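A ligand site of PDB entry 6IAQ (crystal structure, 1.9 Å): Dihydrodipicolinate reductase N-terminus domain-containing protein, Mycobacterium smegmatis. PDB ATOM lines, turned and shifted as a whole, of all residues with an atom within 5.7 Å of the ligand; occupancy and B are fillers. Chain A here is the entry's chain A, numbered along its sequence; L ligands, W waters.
O2 of the ligand sits close to N of Pro 175. Merely in contact with the ligand: Tyr 13 (3.8 Å), Gly 14 (3.9 Å), Ile 37 (3.7 Å), Ala 38 (3.5 Å), Ala 81 (3.6 Å), Val 82 (3.4 Å), Gly 139 (3.8 Å), Phe 173 (3.6 Å), Leu 177 (3.4 Å) and Thr 306 (3.2 Å). Hydrophobic or aromatic side chains that line the ligand: Tyr 13, Ala 17, Met 18, Ile 37, Ala 38, Val 82, Leu 106, Tyr 140, Phe 173, Pro 175 and Leu 177. Within 4 Å of the ligand: Tyr 13, Gly 14, Val 15, Gly 16, Ala 17, Met 18, Ile 37, Ala 38, Arg 39, Ser 40, Lys 43, Ala 81, Val 82, Asn 83, Ser 84, Gln 92, Leu 106, Glu 108, Thr 138, Gly 139, Tyr 140, Gln 141, Phe 173, Gly 174, Pro 175, Glu 176, Leu 177 and Thr 306. The nearest printed residue that does not touch the ligand is Glu 91 (4.3 Å).
An oxygen (O15) of the ligand lies within salt-bridge range of the side-chain amino group (NZ) of Lys 43 (2.6 Å). An oxygen (O12) of the ligand lies within hydrogen-bond range of the backbone NH (N) of Ser 84. The side-chain hydroxyl (OG) of Ser 84 sits at hydrogen-bond distance from an oxygen (O12) of the ligand, at 2.7 Å. An oxygen (O16) of the ligand lies within hydrogen-bond range of the backbone NH (N) of Ser 40. O17 of the ligand lies within hydrogen-bond range of OG of Ser 40 (2.9 Å). OE2 of Glu 108 lies within hydrogen-bond range of O13 of the ligand (2.8 Å). The backbone NH (N) of Gly 174 sits at hydrogen-bond distance from an oxygen (O8) of the ligand. O of Leu 106 lies within hydrogen-bond range of N7 of the ligand (2.9 Å). The backbone NH of Glu 176 sits at hydrogen-bond distance from an oxygen (O2) of the ligand (2.9 Å). An oxygen (O1) of the ligand is in hydrogen-bond range of the backbone NH (N) of Ala 17 (2.9 Å). An oxygen (O14) of the ligand is in hydrogen-bond range of the backbone NH of Tyr 140, 2.9 Å away. A nitrogen (N7) of the ligand is in hydrogen-bond range of the side-chain amide oxygen (OE1) of Gln 141, 2.9 Å away. O12 of the ligand sits close to O of Asn 83. N of Met 18 lies within hydrogen-bond range of O9 of the ligand (3.0 Å). N of Gly 16 sits at hydrogen-bond distance from O5 of the ligand, 3.1 Å away. The backbone NH (N) of Arg 39 lies within hydrogen-bond range of an oxygen (O16) of the ligand, at 3.1 Å. N of Val 15 lies within hydrogen-bond range of O5 of the ligand, at 3.2 Å. The backbone carbonyl oxygen (O) of Thr 138 sits at hydrogen-bond distance from a nitrogen (N7) of the ligand, 3.3 Å away. A nitrogen (N3) of the ligand sits close to the side-chain amide nitrogen (NE2) of Gln 92, at 3.4 Å.
Water W5 lies within hydrogen-bond range of O17 of the ligand (2.6 Å) and NH1 of Arg 39 (3.4 Å). Water W3 lies within hydrogen-bond range of an oxygen (O9) of the ligand (2.7 Å), the backbone carbonyl oxygen of Ala 81 (2.7 Å), the backbone NH of Gly 16 (3.0 Å) and the backbone NH of Asn 19 (3.2 Å). Water W4 lies within hydrogen-bond range of the backbone carbonyl oxygen (O) of Ala 38 (2.4 Å) and a nitrogen (N4) of the ligand (3.2 Å). Water W2 lies within hydrogen-bond range of the side-chain hydroxyl (OH) of Tyr 13 (2.7 Å) and a nitrogen (N3) of the ligand (3.2 Å).
The side-chain carboxylate of Glu 108 is in hydrogen-bond range of the side-chain hydroxyl of Ser 84 (2.6 Å). The side-chain amide oxygen (OE1) of Gln 92 lies within hydrogen-bond range of the side-chain amide nitrogen (ND2) of Asn 83 (3.0 Å). The side-chain hydroxyl (OG) of Ser 107 is in hydrogen-bond range of the backbone carbonyl oxygen (O) of Asn 83, 2.7 Å away. The backbone carbonyl oxygen (O) of Tyr 13 lies within hydrogen-bond range of the backbone NH (N) of Ala 81, 3.0 Å away. The backbone NH (N) of Ala 81 lies close to the side-chain amide nitrogen (ND2) of Asn 19 (3.4 Å). The backbone carbonyl oxygen of Ile 37 sits at hydrogen-bond distance from the backbone NH of Gly 14. The side-chain amide nitrogen (ND2) of Asn 19 lies within hydrogen-bond range of the backbone carbonyl oxygen (O) of Tyr 13, 3.0 Å away. ND2 of Asn 19 sits at hydrogen-bond distance from O of Gly 14.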
ATOM      1  N   TYR A  13     -15.739  -1.390 -17.023  1.00  0.00           N
ATOM      2  CA  TYR A  13     -15.180  -1.039 -15.709  1.00  0.00           C
ATOM      3  C   TYR A  13     -13.791  -0.419 -15.942  1.00  0.00           C
ATOM      4  O   TYR A  13     -12.801  -1.175 -16.205  1.00  0.00           O
ATOM      5  CB  TYR A  13     -15.182  -2.290 -14.843  1.00  0.00           C
ATOM      6  CG  TYR A  13     -15.194  -2.087 -13.353  1.00  0.00           C
ATOM      7  CD1 TYR A  13     -14.611  -0.975 -12.764  1.00  0.00           C
ATOM      8  CD2 TYR A  13     -15.768  -3.036 -12.532  1.00  0.00           C
ATOM      9  CE1 TYR A  13     -14.571  -0.833 -11.389  1.00  0.00           C
ATOM     10  CE2 TYR A  13     -15.768  -2.889 -11.149  1.00  0.00           C
ATOM     11  CZ  TYR A  13     -15.174  -1.779 -10.583  1.00  0.00           C
ATOM     12  OH  TYR A  13     -15.154  -1.625  -9.227  1.00  0.00           O
ATOM     13  N   GLY A  14     -13.723   0.919 -15.823  1.00  0.00           N
ATOM     14  CA  GLY A  14     -12.593   1.737 -16.268  1.00  0.00           C
ATOM     15  C   GLY A  14     -12.817   2.136 -17.703  1.00  0.00           C
ATOM     16  O   GLY A  14     -13.380   1.342 -18.479  1.00  0.00           O
ATOM     17  N   VAL A  15     -12.441   3.361 -18.063  1.00  0.00           N
ATOM     18  CA  VAL A  15     -12.678   3.941 -19.398  1.00  0.00           C
ATOM     19  C   VAL A  15     -11.377   4.616 -19.845  1.00  0.00           C
ATOM     20  O   VAL A  15     -11.420   5.795 -20.242  1.00  0.00           O
ATOM     21  CB  VAL A  15     -13.875   4.902 -19.410  1.00  0.00           C
ATOM     22  CG1 VAL A  15     -14.288   5.174 -20.840  1.00  0.00           C
ATOM     23  CG2 VAL A  15     -15.042   4.341 -18.631  1.00  0.00           C
ATOM     24  N   GLY A  16     -10.271   3.863 -19.801  1.00  0.00           N
ATOM     25  CA  GLY A  16      -8.951   4.427 -20.106  1.00  0.00           C
ATOM     26  C   GLY A  16      -8.509   4.036 -21.481  1.00  0.00           C
ATOM     27  O   GLY A  16      -9.375   3.784 -22.355  1.00  0.00           O
ATOM     28  N   ALA A  17      -7.205   3.964 -21.707  1.00  0.00           N
ATOM     29  CA  ALA A  17      -6.654   3.685 -23.056  1.00  0.00           C
ATOM     30  C   ALA A  17      -7.207   2.338 -23.568  1.00  0.00           C
ATOM     31  O   ALA A  17      -7.670   2.275 -24.741  1.00  0.00           O
ATOM     32  CB  ALA A  17      -5.145   3.673 -22.997  1.00  0.00           C
ATOM     33  N   MET A  18      -7.190   1.294 -22.747  1.00  0.00           N
ATOM     34  CA  MET A  18      -7.583  -0.062 -23.215  1.00  0.00           C
ATOM     35  C   MET A  18      -9.111  -0.168 -23.331  1.00  0.00           C
ATOM     36  O   MET A  18      -9.603  -0.584 -24.390  1.00  0.00           O
ATOM     37  CB  MET A  18      -7.006  -1.183 -22.348  1.00  0.00           C
ATOM     38  CG  MET A  18      -5.464  -1.284 -22.433  1.00  0.00           C
ATOM     39  SD  MET A  18      -4.829  -1.443 -24.116  1.00  0.00           S
ATOM     40  CE  MET A  18      -4.516   0.266 -24.591  1.00  0.00           C
ATOM     41  N   ASN A  19      -9.868   0.213 -22.309  1.00  0.00           N
ATOM     42  CA  ASN A  19     -11.356   0.041 -22.359  1.00  0.00           C
ATOM     43  C   ASN A  19     -11.959   0.946 -23.421  1.00  0.00           C
ATOM     44  O   ASN A  19     -13.039   0.585 -23.923  1.00  0.00           O
ATOM     45  CB  ASN A  19     -12.045   0.137 -21.003  1.00  0.00           C
ATOM     46  CG  ASN A  19     -12.283  -1.222 -20.404  1.00  0.00           C
ATOM     47  OD1 ASN A  19     -12.046  -2.239 -21.084  1.00  0.00           O
ATOM     48  ND2 ASN A  19     -12.720  -1.289 -19.154  1.00  0.00           N
ATOM     49  N   ILE A  37     -17.961   2.613 -15.573  1.00  0.00           N
ATOM     50  CA  ILE A  37     -17.402   3.062 -14.273  1.00  0.00           C
ATOM     51  C   ILE A  37     -16.064   3.755 -14.541  1.00  0.00           C
ATOM     52  O   ILE A  37     -15.209   3.194 -15.283  1.00  0.00           O
ATOM     53  CB  ILE A  37     -17.286   1.903 -13.297  1.00  0.00           C
ATOM     54  CG1 ILE A  37     -18.601   1.116 -13.217  1.00  0.00           C
ATOM     55  CG2 ILE A  37     -16.799   2.380 -11.934  1.00  0.00           C
ATOM     56  CD1 ILE A  37     -18.459  -0.243 -12.599  1.00  0.00           C
ATOM     57  N   ALA A  38     -15.911   4.967 -14.000  1.00  0.00           N
ATOM     58  CA  ALA A  38     -14.676   5.768 -14.077  1.00  0.00           C
ATOM     59  C   ALA A  38     -14.379   6.339 -12.695  1.00  0.00           C
ATOM     60  O   ALA A  38     -15.110   6.020 -11.717  1.00  0.00           O
ATOM     61  CB  ALA A  38     -14.810   6.856 -15.128  1.00  0.00           C
ATOM     62  N   ARG A  39     -13.297   7.111 -12.592  1.00  0.00           N
ATOM     63  CA  ARG A  39     -12.798   7.673 -11.318  1.00  0.00           C
ATOM     64  C   ARG A  39     -12.688   9.196 -11.468  1.00  0.00           C
ATOM     65  O   ARG A  39     -13.007   9.880 -10.509  1.00  0.00           O
ATOM     66  CB  ARG A  39     -11.488   6.963 -10.942  1.00  0.00           C
ATOM     67  CG  ARG A  39     -10.769   7.543  -9.734  1.00  0.00           C
ATOM     68  CD  ARG A  39      -9.588   6.728  -9.319  1.00  0.00           C
ATOM     69  NE  ARG A  39      -9.009   7.332  -8.129  1.00  0.00           N
ATOM     70  CZ  ARG A  39      -8.177   8.371  -8.128  1.00  0.00           C
ATOM     71  NH1 ARG A  39      -7.806   8.947  -9.261  1.00  0.00           N
ATOM     72  NH2 ARG A  39      -7.707   8.823  -6.974  1.00  0.00           N
ATOM     73  N   SER A  40     -12.257   9.720 -12.626  1.00  0.00           N
ATOM     74  CA  SER A  40     -12.025  11.172 -12.871  1.00  0.00           C
ATOM     75  C   SER A  40     -13.350  11.933 -12.901  1.00  0.00           C
ATOM     76  O   SER A  40     -14.257  11.584 -13.667  1.00  0.00           O
ATOM     77  CB  SER A  40     -11.219  11.397 -14.130  1.00  0.00           C
ATOM     78  OG  SER A  40      -9.869  11.008 -13.920  1.00  0.00           O
ATOM     79  N   LYS A  43     -15.275  12.908 -16.074  1.00  0.00           N
ATOM     80  CA  LYS A  43     -15.875  11.818 -16.890  1.00  0.00           C
ATOM     81  C   LYS A  43     -17.249  11.443 -16.361  1.00  0.00           C
ATOM     82  O   LYS A  43     -18.115  11.126 -17.206  1.00  0.00           O
ATOM     83  CB  LYS A  43     -14.955  10.586 -16.915  1.00  0.00           C
ATOM     84  CG  LYS A  43     -13.744  10.824 -17.796  1.00  0.00           C
ATOM     85  CD  LYS A  43     -12.783   9.723 -17.950  1.00  0.00           C
ATOM     86  CE  LYS A  43     -11.577  10.237 -18.710  1.00  0.00           C
ATOM     87  NZ  LYS A  43     -10.499   9.242 -18.715  1.00  0.00           N
ATOM     88  N   ALA A  81     -10.535  -2.864 -17.146  1.00  0.00           N
ATOM     89  CA  ALA A  81      -9.193  -2.370 -17.525  1.00  0.00           C
ATOM     90  C   ALA A  81      -8.845  -1.212 -16.580  1.00  0.00           C
ATOM     91  O   ALA A  81      -8.999  -0.024 -17.021  1.00  0.00           O
ATOM     92  CB  ALA A  81      -9.187  -1.983 -18.960  1.00  0.00           C
ATOM     93  N   VAL A  82      -8.440  -1.518 -15.354  1.00  0.00           N
ATOM     94  CA  VAL A  82      -8.142  -0.424 -14.381  1.00  0.00           C
ATOM     95  C   VAL A  82      -6.739  -0.573 -13.789  1.00  0.00           C
ATOM     96  O   VAL A  82      -6.045   0.428 -13.885  1.00  0.00           O
ATOM     97  CB  VAL A  82      -9.239  -0.144 -13.315  1.00  0.00           C
ATOM     98  CG1 VAL A  82     -10.600  -0.708 -13.671  1.00  0.00           C
ATOM     99  CG2 VAL A  82      -8.826  -0.430 -11.888  1.00  0.00           C
ATOM    100  N   ASN A  83      -6.347  -1.717 -13.242  1.00  0.00           N
ATOM    101  CA  ASN A  83      -5.035  -1.881 -12.560  1.00  0.00           C
ATOM    102  C   ASN A  83      -4.481  -3.302 -12.792  1.00  0.00           C
ATOM    103  O   ASN A  83      -5.145  -4.094 -13.511  1.00  0.00           O
ATOM    104  CB  ASN A  83      -5.138  -1.515 -11.091  1.00  0.00           C
ATOM    105  CG  ASN A  83      -6.262  -2.254 -10.389  1.00  0.00           C
ATOM    106  OD1 ASN A  83      -6.578  -3.386 -10.783  1.00  0.00           O
ATOM    107  ND2 ASN A  83      -6.881  -1.610  -9.400  1.00  0.00           N
ATOM    108  N   SER A  84      -3.326  -3.614 -12.197  1.00  0.00           N
ATOM    109  CA  SER A  84      -2.462  -4.764 -12.581  1.00  0.00           C
ATOM    110  C   SER A  84      -2.389  -5.805 -11.455  1.00  0.00           C
ATOM    111  O   SER A  84      -2.465  -7.007 -11.753  1.00  0.00           O
ATOM    112  CB  SER A  84      -1.081  -4.277 -12.931  1.00  0.00           C
ATOM    113  OG  SER A  84      -1.111  -3.465 -14.102  1.00  0.00           O
ATOM    114  N   GLU A  91     -10.107  -4.922  -4.917  1.00  0.00           N
ATOM    115  CA  GLU A  91     -11.199  -3.957  -4.621  1.00  0.00           C
ATOM    116  C   GLU A  91     -12.283  -4.075  -5.713  1.00  0.00           C
ATOM    117  O   GLU A  91     -13.467  -4.234  -5.329  1.00  0.00           O
ATOM    118  CB  GLU A  91     -10.632  -2.532  -4.513  1.00  0.00           C
ATOM    119  CG  GLU A  91     -11.666  -1.536  -4.035  1.00  0.00           C
ATOM    120  CD  GLU A  91     -11.236  -0.091  -4.178  1.00  0.00           C
ATOM    121  OE1 GLU A  91     -10.093   0.224  -3.787  1.00  0.00           O
ATOM    122  OE2 GLU A  91     -12.014   0.684  -4.749  1.00  0.00           O
ATOM    123  N   GLN A  92     -11.926  -4.022  -7.003  1.00  0.00           N
ATOM    124  CA  GLN A  92     -12.920  -4.099  -8.106  1.00  0.00           C
ATOM    125  C   GLN A  92     -13.467  -5.532  -8.209  1.00  0.00           C
ATOM    126  O   GLN A  92     -14.683  -5.688  -8.477  1.00  0.00           O
ATOM    127  CB  GLN A  92     -12.335  -3.635  -9.436  1.00  0.00           C
ATOM    128  CG  GLN A  92     -11.927  -2.170  -9.415  1.00  0.00           C
ATOM    129  CD  GLN A  92     -10.639  -1.885  -8.696  1.00  0.00           C
ATOM    130  OE1 GLN A  92      -9.672  -2.626  -8.803  1.00  0.00           O
ATOM    131  NE2 GLN A  92     -10.618  -0.765  -7.981  1.00  0.00           N
ATOM    132  N   LEU A 106      -7.907  -7.177 -17.415  1.00  0.00           N
ATOM    133  CA  LEU A 106      -6.530  -7.078 -17.970  1.00  0.00           C
ATOM    134  C   LEU A 106      -5.504  -7.198 -16.861  1.00  0.00           C
ATOM    135  O   LEU A 106      -4.309  -7.225 -17.223  1.00  0.00           O
ATOM    136  CB  LEU A 106      -6.380  -5.738 -18.713  1.00  0.00           C
ATOM    137  CG  LEU A 106      -7.173  -5.647 -20.001  1.00  0.00           C
ATOM    138  CD1 LEU A 106      -6.833  -4.376 -20.721  1.00  0.00           C
ATOM    139  CD2 LEU A 106      -6.991  -6.898 -20.866  1.00  0.00           C
ATOM    140  N   SER A 107      -5.901  -7.228 -15.574  1.00  0.00           N
ATOM    141  CA  SER A 107      -4.926  -7.285 -14.458  1.00  0.00           C
ATOM    142  C   SER A 107      -3.864  -8.367 -14.751  1.00  0.00           C
ATOM    143  O   SER A 107      -4.224  -9.537 -14.792  1.00  0.00           O
ATOM    144  CB  SER A 107      -5.593  -7.497 -13.122  1.00  0.00           C
ATOM    145  OG  SER A 107      -6.367  -6.345 -12.772  1.00  0.00           O
ATOM    146  N   GLU A 108      -2.594  -7.986 -14.896  1.00  0.00           N
ATOM    147  CA  GLU A 108      -1.501  -8.888 -15.336  1.00  0.00           C
ATOM    148  C   GLU A 108      -1.337  -9.996 -14.297  1.00  0.00           C
ATOM    149  O   GLU A 108      -1.083 -11.143 -14.658  1.00  0.00           O
ATOM    150  CB  GLU A 108      -0.193  -8.129 -15.611  1.00  0.00           C
ATOM    151  CG  GLU A 108      -0.263  -7.257 -16.855  1.00  0.00           C
ATOM    152  CD  GLU A 108      -0.727  -5.835 -16.658  1.00  0.00           C
ATOM    153  OE1 GLU A 108      -1.393  -5.564 -15.624  1.00  0.00           O
ATOM    154  OE2 GLU A 108      -0.461  -4.994 -17.558  1.00  0.00           O
ATOM    155  N   THR A 138      -7.026 -11.952 -18.347  1.00  0.00           N
ATOM    156  CA  THR A 138      -6.605 -12.179 -19.743  1.00  0.00           C
ATOM    157  C   THR A 138      -5.908 -10.905 -20.234  1.00  0.00           C
ATOM    158  O   THR A 138      -5.426 -10.120 -19.395  1.00  0.00           O
ATOM    159  CB  THR A 138      -7.790 -12.645 -20.583  1.00  0.00           C
ATOM    160  OG1 THR A 138      -7.400 -12.823 -21.939  1.00  0.00           O
ATOM    161  CG2 THR A 138      -8.949 -11.668 -20.532  1.00  0.00           C
ATOM    162  N   GLY A 139      -5.841 -10.740 -21.552  1.00  0.00           N
ATOM    163  CA  GLY A 139      -5.071  -9.672 -22.219  1.00  0.00           C
ATOM    164  C   GLY A 139      -4.053 -10.269 -23.171  1.00  0.00           C
ATOM    165  O   GLY A 139      -4.266 -11.456 -23.670  1.00  0.00           O
ATOM    166  N   TYR A 140      -2.985  -9.510 -23.426  1.00  0.00           N
ATOM    167  CA  TYR A 140      -1.968  -9.850 -24.457  1.00  0.00           C
ATOM    168  C   TYR A 140      -1.401 -11.252 -24.170  1.00  0.00           C
ATOM    169  O   TYR A 140      -1.261 -12.087 -25.107  1.00  0.00           O
ATOM    170  CB  TYR A 140      -0.856  -8.799 -24.493  1.00  0.00           C
ATOM    171  CG  TYR A 140       0.261  -9.219 -25.425  1.00  0.00           C
ATOM    172  CD1 TYR A 140       0.040  -9.294 -26.787  1.00  0.00           C
ATOM    173  CD2 TYR A 140       1.487  -9.625 -24.923  1.00  0.00           C
ATOM    174  CE1 TYR A 140       1.016  -9.744 -27.655  1.00  0.00           C
ATOM    175  CE2 TYR A 140       2.492 -10.034 -25.781  1.00  0.00           C
ATOM    176  CZ  TYR A 140       2.252 -10.109 -27.143  1.00  0.00           C
ATOM    177  OH  TYR A 140       3.247 -10.530 -27.982  1.00  0.00           O
ATOM    178  N   GLN A 141      -1.086 -11.515 -22.913  1.00  0.00           N
ATOM    179  CA  GLN A 141      -0.293 -12.702 -22.472  1.00  0.00           C
ATOM    180  C   GLN A 141      -1.038 -13.995 -22.821  1.00  0.00           C
ATOM    181  O   GLN A 141      -0.357 -15.029 -23.021  1.00  0.00           O
ATOM    182  CB  GLN A 141       0.017 -12.708 -20.975  1.00  0.00           C
ATOM    183  CG  GLN A 141       0.257 -11.337 -20.331  1.00  0.00           C
ATOM    184  CD  GLN A 141      -1.025 -10.866 -19.695  1.00  0.00           C
ATOM    185  OE1 GLN A 141      -2.017 -10.657 -20.399  1.00  0.00           O
ATOM    186  NE2 GLN A 141      -1.064 -10.862 -18.352  1.00  0.00           N
ATOM    187  N   ASP A 172       1.892   2.956 -25.921  1.00  0.00           N
ATOM    188  CA  ASP A 172       0.695   2.274 -26.484  1.00  0.00           C
ATOM    189  C   ASP A 172      -0.419   2.202 -25.433  1.00  0.00           C
ATOM    190  O   ASP A 172      -1.521   1.826 -25.808  1.00  0.00           O
ATOM    191  CB  ASP A 172       1.013   0.861 -26.985  1.00  0.00           C
ATOM    192  CG  ASP A 172       1.702   0.788 -28.343  1.00  0.00           C
ATOM    193  OD1 ASP A 172       1.754   1.821 -29.049  1.00  0.00           O
ATOM    194  OD2 ASP A 172       2.166  -0.325 -28.687  1.00  0.00           O
ATOM    195  N   PHE A 173      -0.129   2.502 -24.163  1.00  0.00           N
ATOM    196  CA  PHE A 173      -1.033   2.276 -23.000  1.00  0.00           C
ATOM    197  C   PHE A 173      -1.175   3.570 -22.197  1.00  0.00           C
ATOM    198  O   PHE A 173      -0.577   4.610 -22.590  1.00  0.00           O
ATOM    199  CB  PHE A 173      -0.496   1.116 -22.157  1.00  0.00           C
ATOM    200  CG  PHE A 173      -0.245  -0.104 -22.992  1.00  0.00           C
ATOM    201  CD1 PHE A 173      -1.302  -0.868 -23.477  1.00  0.00           C
ATOM    202  CD2 PHE A 173       1.043  -0.453 -23.340  1.00  0.00           C
ATOM    203  CE1 PHE A 173      -1.062  -1.973 -24.279  1.00  0.00           C
ATOM    204  CE2 PHE A 173       1.293  -1.563 -24.150  1.00  0.00           C
ATOM    205  CZ  PHE A 173       0.235  -2.316 -24.618  1.00  0.00           C
ATOM    206  N   GLY A 174      -1.959   3.525 -21.121  1.00  0.00           N
ATOM    207  CA  GLY A 174      -2.389   4.716 -20.389  1.00  0.00           C
ATOM    208  C   GLY A 174      -1.518   5.023 -19.183  1.00  0.00           C
ATOM    209  O   GLY A 174      -0.566   4.292 -18.861  1.00  0.00           O
ATOM    210  N   PRO A 175      -1.846   6.124 -18.463  1.00  0.00           N
ATOM    211  CA  PRO A 175      -1.066   6.578 -17.305  1.00  0.00           C
ATOM    212  C   PRO A 175      -0.873   5.560 -16.179  1.00  0.00           C
ATOM    213  O   PRO A 175       0.187   5.619 -15.500  1.00  0.00           O
ATOM    214  CB  PRO A 175      -1.883   7.763 -16.753  1.00  0.00           C
ATOM    215  CG  PRO A 175      -2.681   8.250 -17.935  1.00  0.00           C
ATOM    216  CD  PRO A 175      -2.969   7.017 -18.773  1.00  0.00           C
ATOM    217  N   GLU A 176      -1.860   4.683 -15.943  1.00  0.00           N
ATOM    218  CA  GLU A 176      -1.747   3.698 -14.839  1.00  0.00           C
ATOM    219  C   GLU A 176      -0.467   2.883 -15.084  1.00  0.00           C
ATOM    220  O   GLU A 176       0.311   2.691 -14.146  1.00  0.00           O
ATOM    221  CB  GLU A 176      -2.991   2.803 -14.762  1.00  0.00           C
ATOM    222  CG  GLU A 176      -2.836   1.632 -13.788  1.00  0.00           C
ATOM    223  CD  GLU A 176      -2.829   2.007 -12.324  1.00  0.00           C
ATOM    224  OE1 GLU A 176      -3.352   3.073 -11.998  1.00  0.00           O
ATOM    225  OE2 GLU A 176      -2.254   1.276 -11.512  1.00  0.00           O
ATOM    226  N   LEU A 177      -0.267   2.389 -16.304  1.00  0.00           N
ATOM    227  CA  LEU A 177       0.855   1.464 -16.612  1.00  0.00           C
ATOM    228  C   LEU A 177       2.160   2.268 -16.702  1.00  0.00           C
ATOM    229  O   LEU A 177       3.156   1.825 -16.146  1.00  0.00           O
ATOM    230  CB  LEU A 177       0.549   0.695 -17.895  1.00  0.00           C
ATOM    231  CG  LEU A 177       1.563  -0.376 -18.302  1.00  0.00           C
ATOM    232  CD1 LEU A 177       1.944  -1.268 -17.146  1.00  0.00           C
ATOM    233  CD2 LEU A 177       1.025  -1.188 -19.467  1.00  0.00           C
ATOM    234  N   PHE A 203       5.175  -9.203 -14.117  1.00  0.00           N
ATOM    235  CA  PHE A 203       4.233  -9.794 -15.098  1.00  0.00           C
ATOM    236  C   PHE A 203       4.710 -11.191 -15.500  1.00  0.00           C
ATOM    237  O   PHE A 203       3.879 -12.122 -15.593  1.00  0.00           O
ATOM    238  CB  PHE A 203       4.103  -8.903 -16.332  1.00  0.00           C
ATOM    239  CG  PHE A 203       3.509  -7.530 -16.082  1.00  0.00           C
ATOM    240  CD1 PHE A 203       3.029  -7.139 -14.837  1.00  0.00           C
ATOM    241  CD2 PHE A 203       3.367  -6.650 -17.144  1.00  0.00           C
ATOM    242  CE1 PHE A 203       2.476  -5.889 -14.651  1.00  0.00           C
ATOM    243  CE2 PHE A 203       2.794  -5.409 -16.953  1.00  0.00           C
ATOM    244  CZ  PHE A 203       2.344  -5.036 -15.720  1.00  0.00           C
ATOM    245  N   THR A 306      -4.215  -7.139 -26.931  1.00  0.00           N
ATOM    246  CA  THR A 306      -4.646  -7.009 -25.521  1.00  0.00           C
ATOM    247  C   THR A 306      -6.187  -6.981 -25.497  1.00  0.00           C
ATOM    248  O   THR A 306      -6.831  -7.743 -24.736  1.00  0.00           O
ATOM    249  CB  THR A 306      -4.085  -5.747 -24.862  1.00  0.00           C
ATOM    250  OG1 THR A 306      -2.686  -5.879 -24.694  1.00  0.00           O
ATOM    251  CG2 THR A 306      -4.746  -5.448 -23.539  1.00  0.00           C
HETATM  252  P1  LIG L   1      -5.283   3.865 -18.174  1.00  0.00           P
HETATM  253  O1  LIG L   1      -5.490   4.498 -19.460  1.00  0.00           O
HETATM  254  O2  LIG L   1      -4.535   4.537 -16.988  1.00  0.00           O
HETATM  255  O3  LIG L   1      -6.767   3.416 -17.649  1.00  0.00           O
HETATM  256  C1  LIG L   1      -7.033   3.029 -16.290  1.00  0.00           C
HETATM  257  C2  LIG L   1      -8.480   3.383 -15.972  1.00  0.00           C
HETATM  258  O4  LIG L   1      -8.845   2.963 -14.665  1.00  0.00           O
HETATM  259  C3  LIG L   1      -8.811   4.905 -16.047  1.00  0.00           C
HETATM  260  O5  LIG L   1      -9.980   4.972 -16.902  1.00  0.00           O
HETATM  261  C4  LIG L   1      -9.194   5.332 -14.634  1.00  0.00           C
HETATM  262  O6  LIG L   1     -10.312   6.251 -14.581  1.00  0.00           O
HETATM  263  C5  LIG L   1      -9.710   4.015 -14.137  1.00  0.00           C
HETATM  264  N1  LIG L   1      -9.749   3.800 -12.692  1.00  0.00           N
HETATM  265  C6  LIG L   1      -8.731   3.839 -11.800  1.00  0.00           C
HETATM  266  N2  LIG L   1      -9.225   3.493 -10.601  1.00  0.00           N
HETATM  267  C7  LIG L   1     -10.520   3.159 -10.759  1.00  0.00           C
HETATM  268  C8  LIG L   1     -11.648   2.675  -9.933  1.00  0.00           C
HETATM  269  N3  LIG L   1     -11.494   2.456  -8.624  1.00  0.00           N
HETATM  270  N4  LIG L   1     -12.839   2.472 -10.501  1.00  0.00           N
HETATM  271  C9  LIG L   1     -13.062   2.657 -11.825  1.00  0.00           C
HETATM  272  N5  LIG L   1     -12.104   3.099 -12.663  1.00  0.00           N
HETATM  273  C10 LIG L   1     -10.873   3.373 -12.150  1.00  0.00           C
HETATM  274  O7  LIG L   1      -4.519   2.422 -18.329  1.00  0.00           O
HETATM  275  P2  LIG L   1      -4.774   1.318 -19.542  1.00  0.00           P
HETATM  276  O8  LIG L   1      -3.730   1.393 -20.608  1.00  0.00           O
HETATM  277  O9  LIG L   1      -6.198   1.335 -19.969  1.00  0.00           O
HETATM  278  O10 LIG L   1      -4.448   0.098 -18.570  1.00  0.00           O
HETATM  279  C11 LIG L   1      -5.279  -0.361 -17.496  1.00  0.00           C
HETATM  280  C12 LIG L   1      -4.739  -1.572 -16.773  1.00  0.00           C
HETATM  281  O11 LIG L   1      -4.748  -2.683 -17.717  1.00  0.00           O
HETATM  282  C13 LIG L   1      -3.348  -1.334 -16.259  1.00  0.00           C
HETATM  283  O12 LIG L   1      -3.152  -1.862 -14.956  1.00  0.00           O
HETATM  284  C14 LIG L   1      -2.478  -2.091 -17.279  1.00  0.00           C
HETATM  285  O13 LIG L   1      -1.233  -2.456 -16.673  1.00  0.00           O
HETATM  286  C15 LIG L   1      -3.433  -3.251 -17.679  1.00  0.00           C
HETATM  287  N6  LIG L   1      -3.101  -3.791 -19.011  1.00  0.00           N
HETATM  288  C16 LIG L   1      -2.949  -5.099 -19.120  1.00  0.00           C
HETATM  289  C17 LIG L   1      -2.578  -5.641 -20.343  1.00  0.00           C
HETATM  290  C18 LIG L   1      -2.444  -7.145 -20.520  1.00  0.00           C
HETATM  291  O14 LIG L   1      -1.956  -7.510 -21.592  1.00  0.00           O
HETATM  292  N7  LIG L   1      -2.880  -8.001 -19.589  1.00  0.00           N
HETATM  293  C19 LIG L   1      -2.390  -4.797 -21.424  1.00  0.00           C
HETATM  294  C20 LIG L   1      -2.552  -3.428 -21.294  1.00  0.00           C
HETATM  295  C21 LIG L   1      -2.923  -2.961 -20.059  1.00  0.00           C
HETATM  296  P3  LIG L   1     -10.245   7.712 -15.225  1.00  0.00           P
HETATM  297  O15 LIG L   1     -10.173   7.582 -16.712  1.00  0.00           O
HETATM  298  O16 LIG L   1     -11.614   8.311 -14.930  1.00  0.00           O
HETATM  299  O17 LIG L   1      -9.029   8.253 -14.455  1.00  0.00           O
HETATM  300  O   HOH W   1      -5.262   6.350 -15.340  1.00  0.00           O
HETATM  301  O   HOH W   2     -14.127   0.670  -8.144  1.00  0.00           O
HETATM  302  O   HOH W   3      -8.845   1.246 -19.455  1.00  0.00           O
HETATM  303  O   HOH W   4     -14.869   4.769  -9.665  1.00  0.00           O
HETATM  304  O   HOH W   5      -7.603   7.593 -12.362  1.00  0.00           O
HETATM  305  O   HOH W   6      -6.334   7.013 -19.931  1.00  0.00           O
HETATM  306  O   HOH W   7      -7.007   8.108 -16.735  1.00  0.00           O
